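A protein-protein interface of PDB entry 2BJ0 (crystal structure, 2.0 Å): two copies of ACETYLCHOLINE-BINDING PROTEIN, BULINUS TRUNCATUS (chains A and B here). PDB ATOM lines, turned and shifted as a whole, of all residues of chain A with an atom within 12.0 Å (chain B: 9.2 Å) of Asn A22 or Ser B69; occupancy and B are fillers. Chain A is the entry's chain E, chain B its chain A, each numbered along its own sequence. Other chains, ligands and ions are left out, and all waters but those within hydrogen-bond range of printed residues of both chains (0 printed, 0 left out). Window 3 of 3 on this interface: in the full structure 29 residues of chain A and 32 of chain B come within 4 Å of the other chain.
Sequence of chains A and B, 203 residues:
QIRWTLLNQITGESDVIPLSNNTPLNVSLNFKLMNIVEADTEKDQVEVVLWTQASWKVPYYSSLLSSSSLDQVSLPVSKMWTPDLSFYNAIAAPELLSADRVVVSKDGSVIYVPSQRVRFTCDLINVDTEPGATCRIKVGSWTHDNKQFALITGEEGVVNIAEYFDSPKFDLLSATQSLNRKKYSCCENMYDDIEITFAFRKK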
ATOM      1  N   VAL A  16      -8.037  34.831  -0.484  1.00  0.00           N
ATOM      2  CA  VAL A  16      -8.134  33.706   0.455  1.00  0.00           C
ATOM      3  C   VAL A  16      -8.315  34.140   1.918  1.00  0.00           C
ATOM      4  O   VAL A  16      -7.686  35.086   2.364  1.00  0.00           O
ATOM      5  CB  VAL A  16      -6.901  32.772   0.295  1.00  0.00           C
ATOM      6  CG1 VAL A  16      -6.986  31.573   1.218  1.00  0.00           C
ATOM      7  CG2 VAL A  16      -6.838  32.264  -1.128  1.00  0.00           C
ATOM      8  N   ILE A  17      -9.223  33.480   2.639  1.00  0.00           N
ATOM      9  CA  ILE A  17      -9.445  33.732   4.065  1.00  0.00           C
ATOM     10  C   ILE A  17      -8.130  33.623   4.862  1.00  0.00           C
ATOM     11  O   ILE A  17      -7.384  32.675   4.697  1.00  0.00           O
ATOM     12  CB  ILE A  17     -10.534  32.769   4.610  1.00  0.00           C
ATOM     13  CG1 ILE A  17     -10.864  33.097   6.056  1.00  0.00           C
ATOM     14  CG2 ILE A  17     -10.108  31.289   4.403  1.00  0.00           C
ATOM     15  CD1 ILE A  17     -12.131  32.447   6.564  1.00  0.00           C
ATOM     16  N   PRO A  18      -7.822  34.637   5.673  1.00  0.00           N
ATOM     17  CA  PRO A  18      -6.564  34.672   6.423  1.00  0.00           C
ATOM     18  C   PRO A  18      -6.567  33.788   7.659  1.00  0.00           C
ATOM     19  O   PRO A  18      -6.971  34.215   8.740  1.00  0.00           O
ATOM     20  CB  PRO A  18      -6.427  36.160   6.802  1.00  0.00           C
ATOM     21  CG  PRO A  18      -7.848  36.636   6.913  1.00  0.00           C
ATOM     22  CD  PRO A  18      -8.624  35.856   5.872  1.00  0.00           C
ATOM     23  N   LEU A  19      -6.107  32.558   7.503  1.00  0.00           N
ATOM     24  CA  LEU A  19      -5.975  31.656   8.641  1.00  0.00           C
ATOM     25  C   LEU A  19      -4.549  31.637   9.230  1.00  0.00           C
ATOM     26  O   LEU A  19      -3.564  31.757   8.484  1.00  0.00           O
ATOM     27  CB  LEU A  19      -6.379  30.233   8.232  1.00  0.00           C
ATOM     28  CG  LEU A  19      -7.799  30.050   7.709  1.00  0.00           C
ATOM     29  CD1 LEU A  19      -8.109  28.580   7.487  1.00  0.00           C
ATOM     30  CD2 LEU A  19      -8.790  30.651   8.663  1.00  0.00           C
ATOM     31  N   SER A  20      -4.459  31.492  10.559  1.00  0.00           N
ATOM     32  CA  SER A  20      -3.214  31.131  11.256  1.00  0.00           C
ATOM     33  C   SER A  20      -3.224  29.630  11.574  1.00  0.00           C
ATOM     34  O   SER A  20      -3.999  29.166  12.429  1.00  0.00           O
ATOM     35  CB  SER A  20      -3.069  31.904  12.569  1.00  0.00           C
ATOM     36  OG  SER A  20      -2.884  33.298  12.349  1.00  0.00           O
ATOM     37  N   ASN A  21      -2.368  28.874  10.885  1.00  0.00           N
ATOM     38  CA  ASN A  21      -2.320  27.419  11.054  1.00  0.00           C
ATOM     39  C   ASN A  21      -3.653  26.782  10.612  1.00  0.00           C
ATOM     40  O   ASN A  21      -4.186  27.145   9.560  1.00  0.00           O
ATOM     41  CB  ASN A  21      -1.973  27.055  12.505  1.00  0.00           C
ATOM     42  CG  ASN A  21      -0.502  27.344  12.863  1.00  0.00           C
ATOM     43  OD1 ASN A  21       0.297  26.411  13.037  1.00  0.00           O
ATOM     44  ND2 ASN A  21      -0.145  28.629  12.977  1.00  0.00           N
ATOM     45  N   ASN A  22      -4.195  25.861  11.411  1.00  0.00           N
ATOM     46  CA  ASN A  22      -5.441  25.160  11.053  1.00  0.00           C
ATOM     47  C   ASN A  22      -6.721  25.798  11.594  1.00  0.00           C
ATOM     48  O   ASN A  22      -7.806  25.580  11.043  1.00  0.00           O
ATOM     49  CB  ASN A  22      -5.395  23.681  11.488  1.00  0.00           C
ATOM     50  CG  ASN A  22      -5.014  22.742  10.348  1.00  0.00           C
ATOM     51  OD1 ASN A  22      -4.036  22.980   9.642  1.00  0.00           O
ATOM     52  ND2 ASN A  22      -5.783  21.659  10.176  1.00  0.00           N
ATOM     53  N   THR A  23      -6.582  26.568  12.676  1.00  0.00           N
ATOM     54  CA  THR A  23      -7.710  27.149  13.405  1.00  0.00           C
ATOM     55  C   THR A  23      -8.603  27.950  12.478  1.00  0.00           C
ATOM     56  O   THR A  23      -8.091  28.703  11.664  1.00  0.00           O
ATOM     57  CB  THR A  23      -7.189  28.071  14.530  1.00  0.00           C
ATOM     58  OG1 THR A  23      -6.056  27.461  15.164  1.00  0.00           O
ATOM     59  CG2 THR A  23      -8.216  28.185  15.646  1.00  0.00           C
ATOM     60  N   PRO A  24      -9.924  27.770  12.584  1.00  0.00           N
ATOM     61  CA  PRO A  24     -10.875  28.624  11.865  1.00  0.00           C
ATOM     62  C   PRO A  24     -10.818  30.065  12.364  1.00  0.00           C
ATOM     63  O   PRO A  24     -10.503  30.305  13.525  1.00  0.00           O
ATOM     64  CB  PRO A  24     -12.241  28.002  12.179  1.00  0.00           C
ATOM     65  CG  PRO A  24     -12.029  27.143  13.382  1.00  0.00           C
ATOM     66  CD  PRO A  24     -10.600  26.710  13.353  1.00  0.00           C
ATOM     67  N   LEU A  25     -11.121  30.995  11.468  1.00  0.00           N
ATOM     68  CA  LEU A  25     -11.144  32.417  11.768  1.00  0.00           C
ATOM     69  C   LEU A  25     -12.414  32.749  12.514  1.00  0.00           C
ATOM     70  O   LEU A  25     -13.515  32.420  12.058  1.00  0.00           O
ATOM     71  CB  LEU A  25     -11.112  33.203  10.452  1.00  0.00           C
ATOM     72  CG  LEU A  25     -10.994  34.727  10.535  1.00  0.00           C
ATOM     73  CD1 LEU A  25      -9.641  35.109  11.097  1.00  0.00           C
ATOM     74  CD2 LEU A  25     -11.209  35.352   9.178  1.00  0.00           C
ATOM     75  N   ASN A  26     -12.270  33.413  13.652  1.00  0.00           N
ATOM     76  CA  ASN A  26     -13.399  33.872  14.420  1.00  0.00           C
ATOM     77  C   ASN A  26     -13.897  35.146  13.814  1.00  0.00           C
ATOM     78  O   ASN A  26     -13.165  36.133  13.793  1.00  0.00           O
ATOM     79  CB  ASN A  26     -12.980  34.175  15.850  1.00  0.00           C
ATOM     80  CG  ASN A  26     -13.052  32.975  16.755  1.00  0.00           C
ATOM     81  OD1 ASN A  26     -13.552  31.902  16.370  1.00  0.00           O
ATOM     82  ND2 ASN A  26     -12.563  33.148  17.991  1.00  0.00           N
ATOM     83  N   LYS A  57      -9.737  39.189  13.368  1.00  0.00           N
ATOM     84  CA  LYS A  57      -8.361  39.612  13.646  1.00  0.00           C
ATOM     85  C   LYS A  57      -7.423  38.887  12.753  1.00  0.00           C
ATOM     86  O   LYS A  57      -7.584  37.682  12.545  1.00  0.00           O
ATOM     87  CB  LYS A  57      -7.977  39.366  15.108  1.00  0.00           C
ATOM     88  CG  LYS A  57      -6.688  40.129  15.553  1.00  0.00           C
ATOM     89  CD  LYS A  57      -6.626  40.298  17.075  1.00  0.00           C
ATOM     90  CE  LYS A  57      -5.180  40.311  17.563  1.00  0.00           C
ATOM     91  NZ  LYS A  57      -5.064  40.310  19.067  1.00  0.00           N
ATOM     92  N   PRO A  59      -3.443  38.844  13.007  1.00  0.00           N
ATOM     93  CA  PRO A  59      -2.243  39.339  13.694  1.00  0.00           C
ATOM     94  C   PRO A  59      -1.164  39.985  12.798  1.00  0.00           C
ATOM     95  O   PRO A  59      -0.658  41.067  13.151  1.00  0.00           O
ATOM     96  CB  PRO A  59      -1.718  38.089  14.412  1.00  0.00           C
ATOM     97  CG  PRO A  59      -3.003  37.335  14.780  1.00  0.00           C
ATOM     98  CD  PRO A  59      -3.875  37.534  13.541  1.00  0.00           C
ATOM     99  N   HIS A 144     -17.541  29.709   2.969  1.00  0.00           N
ATOM    100  CA  HIS A 144     -16.546  29.282   3.979  1.00  0.00           C
ATOM    101  C   HIS A 144     -17.239  28.469   5.066  1.00  0.00           C
ATOM    102  O   HIS A 144     -17.974  29.016   5.862  1.00  0.00           O
ATOM    103  CB  HIS A 144     -15.779  30.484   4.592  1.00  0.00           C
ATOM    104  CG  HIS A 144     -14.938  31.227   3.598  1.00  0.00           C
ATOM    105  ND1 HIS A 144     -15.366  32.372   2.954  1.00  0.00           N
ATOM    106  CD2 HIS A 144     -13.695  30.972   3.125  1.00  0.00           C
ATOM    107  CE1 HIS A 144     -14.424  32.782   2.122  1.00  0.00           C
ATOM    108  NE2 HIS A 144     -13.395  31.954   2.215  1.00  0.00           N
ATOM    109  N   ASP A 145     -17.030  27.153   5.076  1.00  0.00           N
ATOM    110  CA  ASP A 145     -17.686  26.297   6.068  1.00  0.00           C
ATOM    111  C   ASP A 145     -17.073  26.518   7.413  1.00  0.00           C
ATOM    112  O   ASP A 145     -16.109  27.265   7.530  1.00  0.00           O
ATOM    113  CB  ASP A 145     -17.668  24.821   5.668  1.00  0.00           C
ATOM    114  CG  ASP A 145     -16.277  24.238   5.595  1.00  0.00           C
ATOM    115  OD1 ASP A 145     -15.367  24.651   6.330  1.00  0.00           O
ATOM    116  OD2 ASP A 145     -16.003  23.316   4.814  1.00  0.00           O
ATOM    117  N   ASN A 146     -17.627  25.879   8.437  1.00  0.00           N
ATOM    118  CA  ASN A 146     -17.265  26.225   9.803  1.00  0.00           C
ATOM    119  C   ASN A 146     -15.884  25.742  10.267  1.00  0.00           C
ATOM    120  O   ASN A 146     -15.403  26.134  11.333  1.00  0.00           O
ATOM    121  CB  ASN A 146     -18.406  25.878  10.773  1.00  0.00           C
ATOM    122  CG  ASN A 146     -18.281  24.507  11.359  1.00  0.00           C
ATOM    123  OD1 ASN A 146     -18.294  24.366  12.570  1.00  0.00           O
ATOM    124  ND2 ASN A 146     -18.137  23.481  10.510  1.00  0.00           N
ATOM    125  N   LYS A 147     -15.227  24.947   9.432  1.00  0.00           N
ATOM    126  CA  LYS A 147     -13.813  24.566   9.655  1.00  0.00           C
ATOM    127  C   LYS A 147     -12.878  25.714   9.308  1.00  0.00           C
ATOM    128  O   LYS A 147     -11.713  25.696   9.685  1.00  0.00           O
ATOM    129  CB  LYS A 147     -13.425  23.372   8.780  1.00  0.00           C
ATOM    130  CG  LYS A 147     -14.106  22.068   9.188  1.00  0.00           C
ATOM    131  CD  LYS A 147     -13.960  21.001   8.115  1.00  0.00           C
ATOM    132  CE  LYS A 147     -14.713  19.720   8.560  1.00  0.00           C
ATOM    133  NZ  LYS A 147     -13.987  18.470   8.133  1.00  0.00           N
ATOM    134  N   GLN A 148     -13.369  26.688   8.557  1.00  0.00           N
ATOM    135  CA  GLN A 148     -12.529  27.827   8.180  1.00  0.00           C
ATOM    136  C   GLN A 148     -13.004  29.138   8.796  1.00  0.00           C
ATOM    137  O   GLN A 148     -12.207  30.028   9.084  1.00  0.00           O
ATOM    138  CB  GLN A 148     -12.430  27.943   6.648  1.00  0.00           C
ATOM    139  CG  GLN A 148     -11.465  26.958   6.038  1.00  0.00           C
ATOM    140  CD  GLN A 148     -11.449  27.001   4.519  1.00  0.00           C
ATOM    141  OE1 GLN A 148     -11.660  28.047   3.916  1.00  0.00           O
ATOM    142  NE2 GLN A 148     -11.180  25.859   3.900  1.00  0.00           N
ATOM    143  N   PHE A 149     -14.311  29.238   8.989  1.00  0.00           N
ATOM    144  CA  PHE A 149     -14.963  30.506   9.267  1.00  0.00           C
ATOM    145  C   PHE A 149     -15.944  30.267  10.394  1.00  0.00           C
ATOM    146  O   PHE A 149     -17.004  29.691  10.205  1.00  0.00           O
ATOM    147  CB  PHE A 149     -15.658  30.960   7.970  1.00  0.00           C
ATOM    148  CG  PHE A 149     -16.352  32.306   8.030  1.00  0.00           C
ATOM    149  CD1 PHE A 149     -17.554  32.467   8.724  1.00  0.00           C
ATOM    150  CD2 PHE A 149     -15.875  33.371   7.265  1.00  0.00           C
ATOM    151  CE1 PHE A 149     -18.239  33.688   8.737  1.00  0.00           C
ATOM    152  CE2 PHE A 149     -16.561  34.601   7.259  1.00  0.00           C
ATOM    153  CZ  PHE A 149     -17.752  34.752   7.997  1.00  0.00           C
ATOM    154  N   ALA A 150     -15.584  30.721  11.586  1.00  0.00           N
ATOM    155  CA  ALA A 150     -16.411  30.506  12.755  1.00  0.00           C
ATOM    156  C   ALA A 150     -17.156  31.777  13.154  1.00  0.00           C
ATOM    157  O   ALA A 150     -16.532  32.794  13.480  1.00  0.00           O
ATOM    158  CB  ALA A 150     -15.546  30.008  13.896  1.00  0.00           C
ATOM    159  N   GLU A 188     -20.429  19.318   1.527  1.00  0.00           N
ATOM    160  CA  GLU A 188     -19.917  18.396   2.557  1.00  0.00           C
ATOM    161  C   GLU A 188     -20.070  18.830   4.011  1.00  0.00           C
ATOM    162  O   GLU A 188     -20.521  18.046   4.869  1.00  0.00           O
ATOM    163  CB  GLU A 188     -18.420  18.179   2.337  1.00  0.00           C
ATOM    164  CG  GLU A 188     -18.039  16.982   1.496  1.00  0.00           C
ATOM    165  CD  GLU A 188     -16.532  16.843   1.404  1.00  0.00           C
ATOM    166  OE1 GLU A 188     -15.837  17.851   1.693  1.00  0.00           O
ATOM    167  OE2 GLU A 188     -16.043  15.740   1.053  1.00  0.00           O
ATOM    168  N   ASN A 189     -19.634  20.056   4.301  1.00  0.00           N
ATOM    169  CA  ASN A 189     -19.504  20.503   5.687  1.00  0.00           C
ATOM    170  C   ASN A 189     -20.666  21.351   6.166  1.00  0.00           C
ATOM    171  O   ASN A 189     -21.646  21.555   5.443  1.00  0.00           O
ATOM    172  CB  ASN A 189     -18.174  21.223   5.902  1.00  0.00           C
ATOM    173  CG  ASN A 189     -16.967  20.293   5.772  1.00  0.00           C
ATOM    174  OD1 ASN A 189     -16.934  19.208   6.357  1.00  0.00           O
ATOM    175  ND2 ASN A 189     -15.970  20.722   5.006  1.00  0.00           N
ATOM    176  N   GLN B   1      -0.768  31.130   1.597  1.00  0.00           N
ATOM    177  CA  GLN B   1      -1.788  30.127   2.071  1.00  0.00           C
ATOM    178  C   GLN B   1      -2.008  28.945   1.075  1.00  0.00           C
ATOM    179  O   GLN B   1      -2.404  27.854   1.477  1.00  0.00           O
ATOM    180  CB  GLN B   1      -3.113  30.837   2.352  1.00  0.00           C
ATOM    181  CG  GLN B   1      -2.993  32.126   3.179  1.00  0.00           C
ATOM    182  CD  GLN B   1      -3.553  31.981   4.607  1.00  0.00           C
ATOM    183  OE1 GLN B   1      -3.044  32.609   5.550  1.00  0.00           O
ATOM    184  NE2 GLN B   1      -4.606  31.154   4.765  1.00  0.00           N
ATOM    185  N   ILE B   2      -1.753  29.194  -0.210  1.00  0.00           N
ATOM    186  CA  ILE B   2      -1.932  28.244  -1.315  1.00  0.00           C
ATOM    187  C   ILE B   2      -0.774  28.489  -2.299  1.00  0.00           C
ATOM    188  O   ILE B   2       0.015  29.444  -2.121  1.00  0.00           O
ATOM    189  CB  ILE B   2      -3.269  28.527  -2.045  1.00  0.00           C
ATOM    190  CG1 ILE B   2      -3.333  29.991  -2.489  1.00  0.00           C
ATOM    191  CG2 ILE B   2      -4.478  28.190  -1.163  1.00  0.00           C
ATOM    192  CD1 ILE B   2      -4.468  30.311  -3.468  1.00  0.00           C
ATOM    193  N   LEU B  64      -3.036  23.354  -6.207  1.00  0.00           N
ATOM    194  CA  LEU B  64      -3.266  24.615  -5.542  1.00  0.00           C
ATOM    195  C   LEU B  64      -3.175  24.391  -4.046  1.00  0.00           C
ATOM    196  O   LEU B  64      -2.755  25.275  -3.308  1.00  0.00           O
ATOM    197  CB  LEU B  64      -4.644  25.161  -5.935  1.00  0.00           C
ATOM    198  CG  LEU B  64      -4.985  26.648  -5.809  1.00  0.00           C
ATOM    199  CD1 LEU B  64      -4.043  27.589  -6.602  1.00  0.00           C
ATOM    200  CD2 LEU B  64      -6.432  26.836  -6.258  1.00  0.00           C
ATOM    201  N   LEU B  65      -3.540  23.189  -3.616  1.00  0.00           N
ATOM    202  CA  LEU B  65      -3.698  22.877  -2.198  1.00  0.00           C
ATOM    203  C   LEU B  65      -2.757  21.817  -1.637  1.00  0.00           C
ATOM    204  O   LEU B  65      -2.452  21.853  -0.448  1.00  0.00           O
ATOM    205  CB  LEU B  65      -5.137  22.433  -1.914  1.00  0.00           C
ATOM    206  CG  LEU B  65      -6.211  23.518  -1.953  1.00  0.00           C
ATOM    207  CD1 LEU B  65      -7.527  22.910  -1.529  1.00  0.00           C
ATOM    208  CD2 LEU B  65      -5.844  24.724  -1.068  1.00  0.00           C
ATOM    209  N   SER B  66      -2.329  20.879  -2.481  1.00  0.00           N
ATOM    210  CA  SER B  66      -1.568  19.677  -2.087  1.00  0.00           C
ATOM    211  C   SER B  66      -0.590  19.799  -0.884  1.00  0.00           C
ATOM    212  O   SER B  66      -0.387  18.822  -0.146  1.00  0.00           O
ATOM    213  CB  SER B  66      -0.862  19.071  -3.311  1.00  0.00           C
ATOM    214  OG  SER B  66      -0.096  20.059  -3.984  1.00  0.00           O
ATOM    215  N   SER B  67      -0.007  20.986  -0.691  1.00  0.00           N
ATOM    216  CA  SER B  67       0.882  21.234   0.448  1.00  0.00           C
ATOM    217  C   SER B  67       0.413  22.379   1.361  1.00  0.00           C
ATOM    218  O   SER B  67       1.216  23.166   1.870  1.00  0.00           O
ATOM    219  CB  SER B  67       2.309  21.489  -0.047  1.00  0.00           C
ATOM    220  OG  SER B  67       2.321  22.547  -0.988  1.00  0.00           O
ATOM    221  N   SER B  68      -0.893  22.467   1.577  1.00  0.00           N
ATOM    222  CA  SER B  68      -1.433  23.437   2.514  1.00  0.00           C
ATOM    223  C   SER B  68      -2.391  22.722   3.461  1.00  0.00           C
ATOM    224  O   SER B  68      -2.887  21.614   3.159  1.00  0.00           O
ATOM    225  CB  SER B  68      -2.127  24.594   1.781  1.00  0.00           C
ATOM    226  OG  SER B  68      -3.434  24.237   1.381  1.00  0.00           O
ATOM    227  N   SER B  69      -2.637  23.351   4.609  1.00  0.00           N
ATOM    228  CA  SER B  69      -3.506  22.786   5.631  1.00  0.00           C
ATOM    229  C   SER B  69      -4.936  22.666   5.116  1.00  0.00           C
ATOM    230  O   SER B  69      -5.580  21.616   5.301  1.00  0.00           O
ATOM    231  CB  SER B  69      -3.444  23.631   6.902  1.00  0.00           C
ATOM    232  OG  SER B  69      -2.875  24.913   6.649  1.00  0.00           O
ATOM    233  N   LEU B  70      -5.392  23.732   4.441  1.00  0.00           N
ATOM    234  CA  LEU B  70      -6.730  23.836   3.828  1.00  0.00           C
ATOM    235  C   LEU B  70      -7.134  22.590   3.025  1.00  0.00           C
ATOM    236  O   LEU B  70      -6.376  22.147   2.165  1.00  0.00           O
ATOM    237  CB  LEU B  70      -6.788  25.072   2.907  1.00  0.00           C
ATOM    238  CG  LEU B  70      -6.509  26.492   3.416  1.00  0.00           C
ATOM    239  CD1 LEU B  70      -6.605  27.482   2.287  1.00  0.00           C
ATOM    240  CD2 LEU B  70      -7.464  26.899   4.504  1.00  0.00           C
ATOM    241  N   ASP B  71      -8.322  22.049   3.302  1.00  0.00           N
ATOM    242  CA  ASP B  71      -8.877  20.913   2.536  1.00  0.00           C
ATOM    243  C   ASP B  71      -9.574  21.387   1.265  1.00  0.00           C
ATOM    244  O   ASP B  71      -9.772  20.616   0.317  1.00  0.00           O
ATOM    245  CB  ASP B  71      -9.869  20.094   3.384  1.00  0.00           C
ATOM    246  CG  ASP B  71      -9.358  19.841   4.802  1.00  0.00           C
ATOM    247  OD1 ASP B  71      -8.172  19.422   4.942  1.00  0.00           O
ATOM    248  OD2 ASP B  71     -10.061  20.055   5.832  1.00  0.00           O
ATOM    249  N   GLN B  72      -9.978  22.650   1.282  1.00  0.00           N
ATOM    250  CA  GLN B  72     -10.535  23.318   0.122  1.00  0.00           C
ATOM    251  C   GLN B  72     -10.340  24.827   0.267  1.00  0.00           C
ATOM    252  O   GLN B  72      -9.980  25.308   1.344  1.00  0.00           O
ATOM    253  CB  GLN B  72     -12.004  22.984  -0.038  1.00  0.00           C
ATOM    254  CG  GLN B  72     -12.816  23.202   1.207  1.00  0.00           C
ATOM    255  CD  GLN B  72     -14.203  22.663   1.046  1.00  0.00           C
ATOM    256  OE1 GLN B  72     -14.393  21.568   0.481  1.00  0.00           O
ATOM    257  NE2 GLN B  72     -15.191  23.417   1.525  1.00  0.00           N
ATOM    258  N   VAL B  73     -10.525  25.545  -0.838  1.00  0.00           N
ATOM    259  CA  VAL B  73     -10.328  26.983  -0.845  1.00  0.00           C
ATOM    260  C   VAL B  73     -11.437  27.613  -1.669  1.00  0.00           C
ATOM    261  O   VAL B  73     -11.808  27.114  -2.746  1.00  0.00           O
ATOM    262  CB  VAL B  73      -8.872  27.403  -1.313  1.00  0.00           C
ATOM    263  CG1 VAL B  73      -8.642  27.130  -2.745  1.00  0.00           C
ATOM    264  CG2 VAL B  73      -8.583  28.895  -1.005  1.00  0.00           C
ATOM    265  N   LYS B 106      -9.255  19.598  -2.945  1.00  0.00           N
ATOM    266  CA  LYS B 106      -7.880  19.068  -3.094  1.00  0.00           C
ATOM    267  C   LYS B 106      -7.646  18.296  -4.379  1.00  0.00           C
ATOM    268  O   LYS B 106      -6.531  18.247  -4.870  1.00  0.00           O
ATOM    269  CB  LYS B 106      -7.475  18.174  -1.907  1.00  0.00           C
ATOM    270  CG  LYS B 106      -7.115  18.952  -0.629  1.00  0.00           C
ATOM    271  CD  LYS B 106      -5.763  18.535  -0.001  1.00  0.00           C
ATOM    272  CE  LYS B 106      -5.455  19.464   1.202  1.00  0.00           C
ATOM    273  NZ  LYS B 106      -4.007  19.824   1.378  1.00  0.00           N
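The backbone carbonyl oxygen (O) of Ile A17 sits at hydrogen-bond distance from the side-chain amide nitrogen (NE2) of Gln B1.
OE1 of Gln B1 lies close to O of Leu A19 (3.1 Å).
The side-chain amide nitrogen of Gln B72 is in hydrogen-bond range of the side-chain carboxylate of Asp A145, at 3.4 Å.
The side-chain amide nitrogen (NE2) of Gln A148 lies within hydrogen-bond range of the backbone carbonyl oxygen (O) of Gln B72 (2.9 Å).
The backbone carbonyl oxygen (O) of Leu B70 lies close to the side-chain amino group (NZ) of Lys B106 (3.4 Å).
The backbone NH (N) of Leu A25 is in hydrogen-bond range of the backbone carbonyl oxygen (O) of Gln A148 (2.8 Å).
OD1 of Asp A145 lies within hydrogen-bond range of N of Lys A147 (3.1 Å).
The side-chain carboxylate of Asp A145 is in hydrogen-bond range of the side-chain amide nitrogen of Asn A189, at 2.6 Å.
Ile B2 touches Val A16.
CG2 of Val A16 touches CG2 of Val B73 (3.8 Å).
CD1 of Leu A19 touches CD2 of Leu B70 (3.5 Å).
O of Asn A21 touches OG of Ser B69, 3.9 Å away.
Ser B69 touches Asn A22.
Gln A148 touches Leu B70 (NE2 to CD2, 3.9 Å).
Asn A22 touches just one residue of chain B: Ser B69 (2.9 Å).
No residue of chain B comes within 4 Å of Thr A23.
His A144 touches none of the printed residues of chain B.
Asn A146 touches none of the printed residues of chain B.
Of the printed residues of chain A, Gln B1 touches Ile A17 and Leu A19.
No residue of chain A comes within 4 Å of Ser B67.
Ser B68 touches none of the printed residues of chain A.
Leu B70 touches just these residues of chain A: Leu A19 (3.5 Å) and Gln A148 (3.9 Å).
No residue of chain A comes within 4 Å of Asp B71.
Printed residues of chain A within 4 Å of Gln B72: Asp A145 and Gln A148.
Of the printed residues of chain A, Val B73 touches Val A16 (3.8 Å).
The nearest residue of chain A that does not touch Ser B69 is Leu A19 (6.4 Å).
The nearest printed residue of chain A that does not touch Ile B2 is Ile A17 (7.9 Å).
Hydrophobic or aromatic side chains of chain B within 4 Å of the printed part of chain A: Ile B2, Leu B70 and Val B73.
Along chain B the printed residues that touch a printed residue of chain A span positions 1 to 73.
No position is printed for both chains.
Of the 10 pairs that touch across the chains among the printed residues, none has its exchanged pair printed and touching as well.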
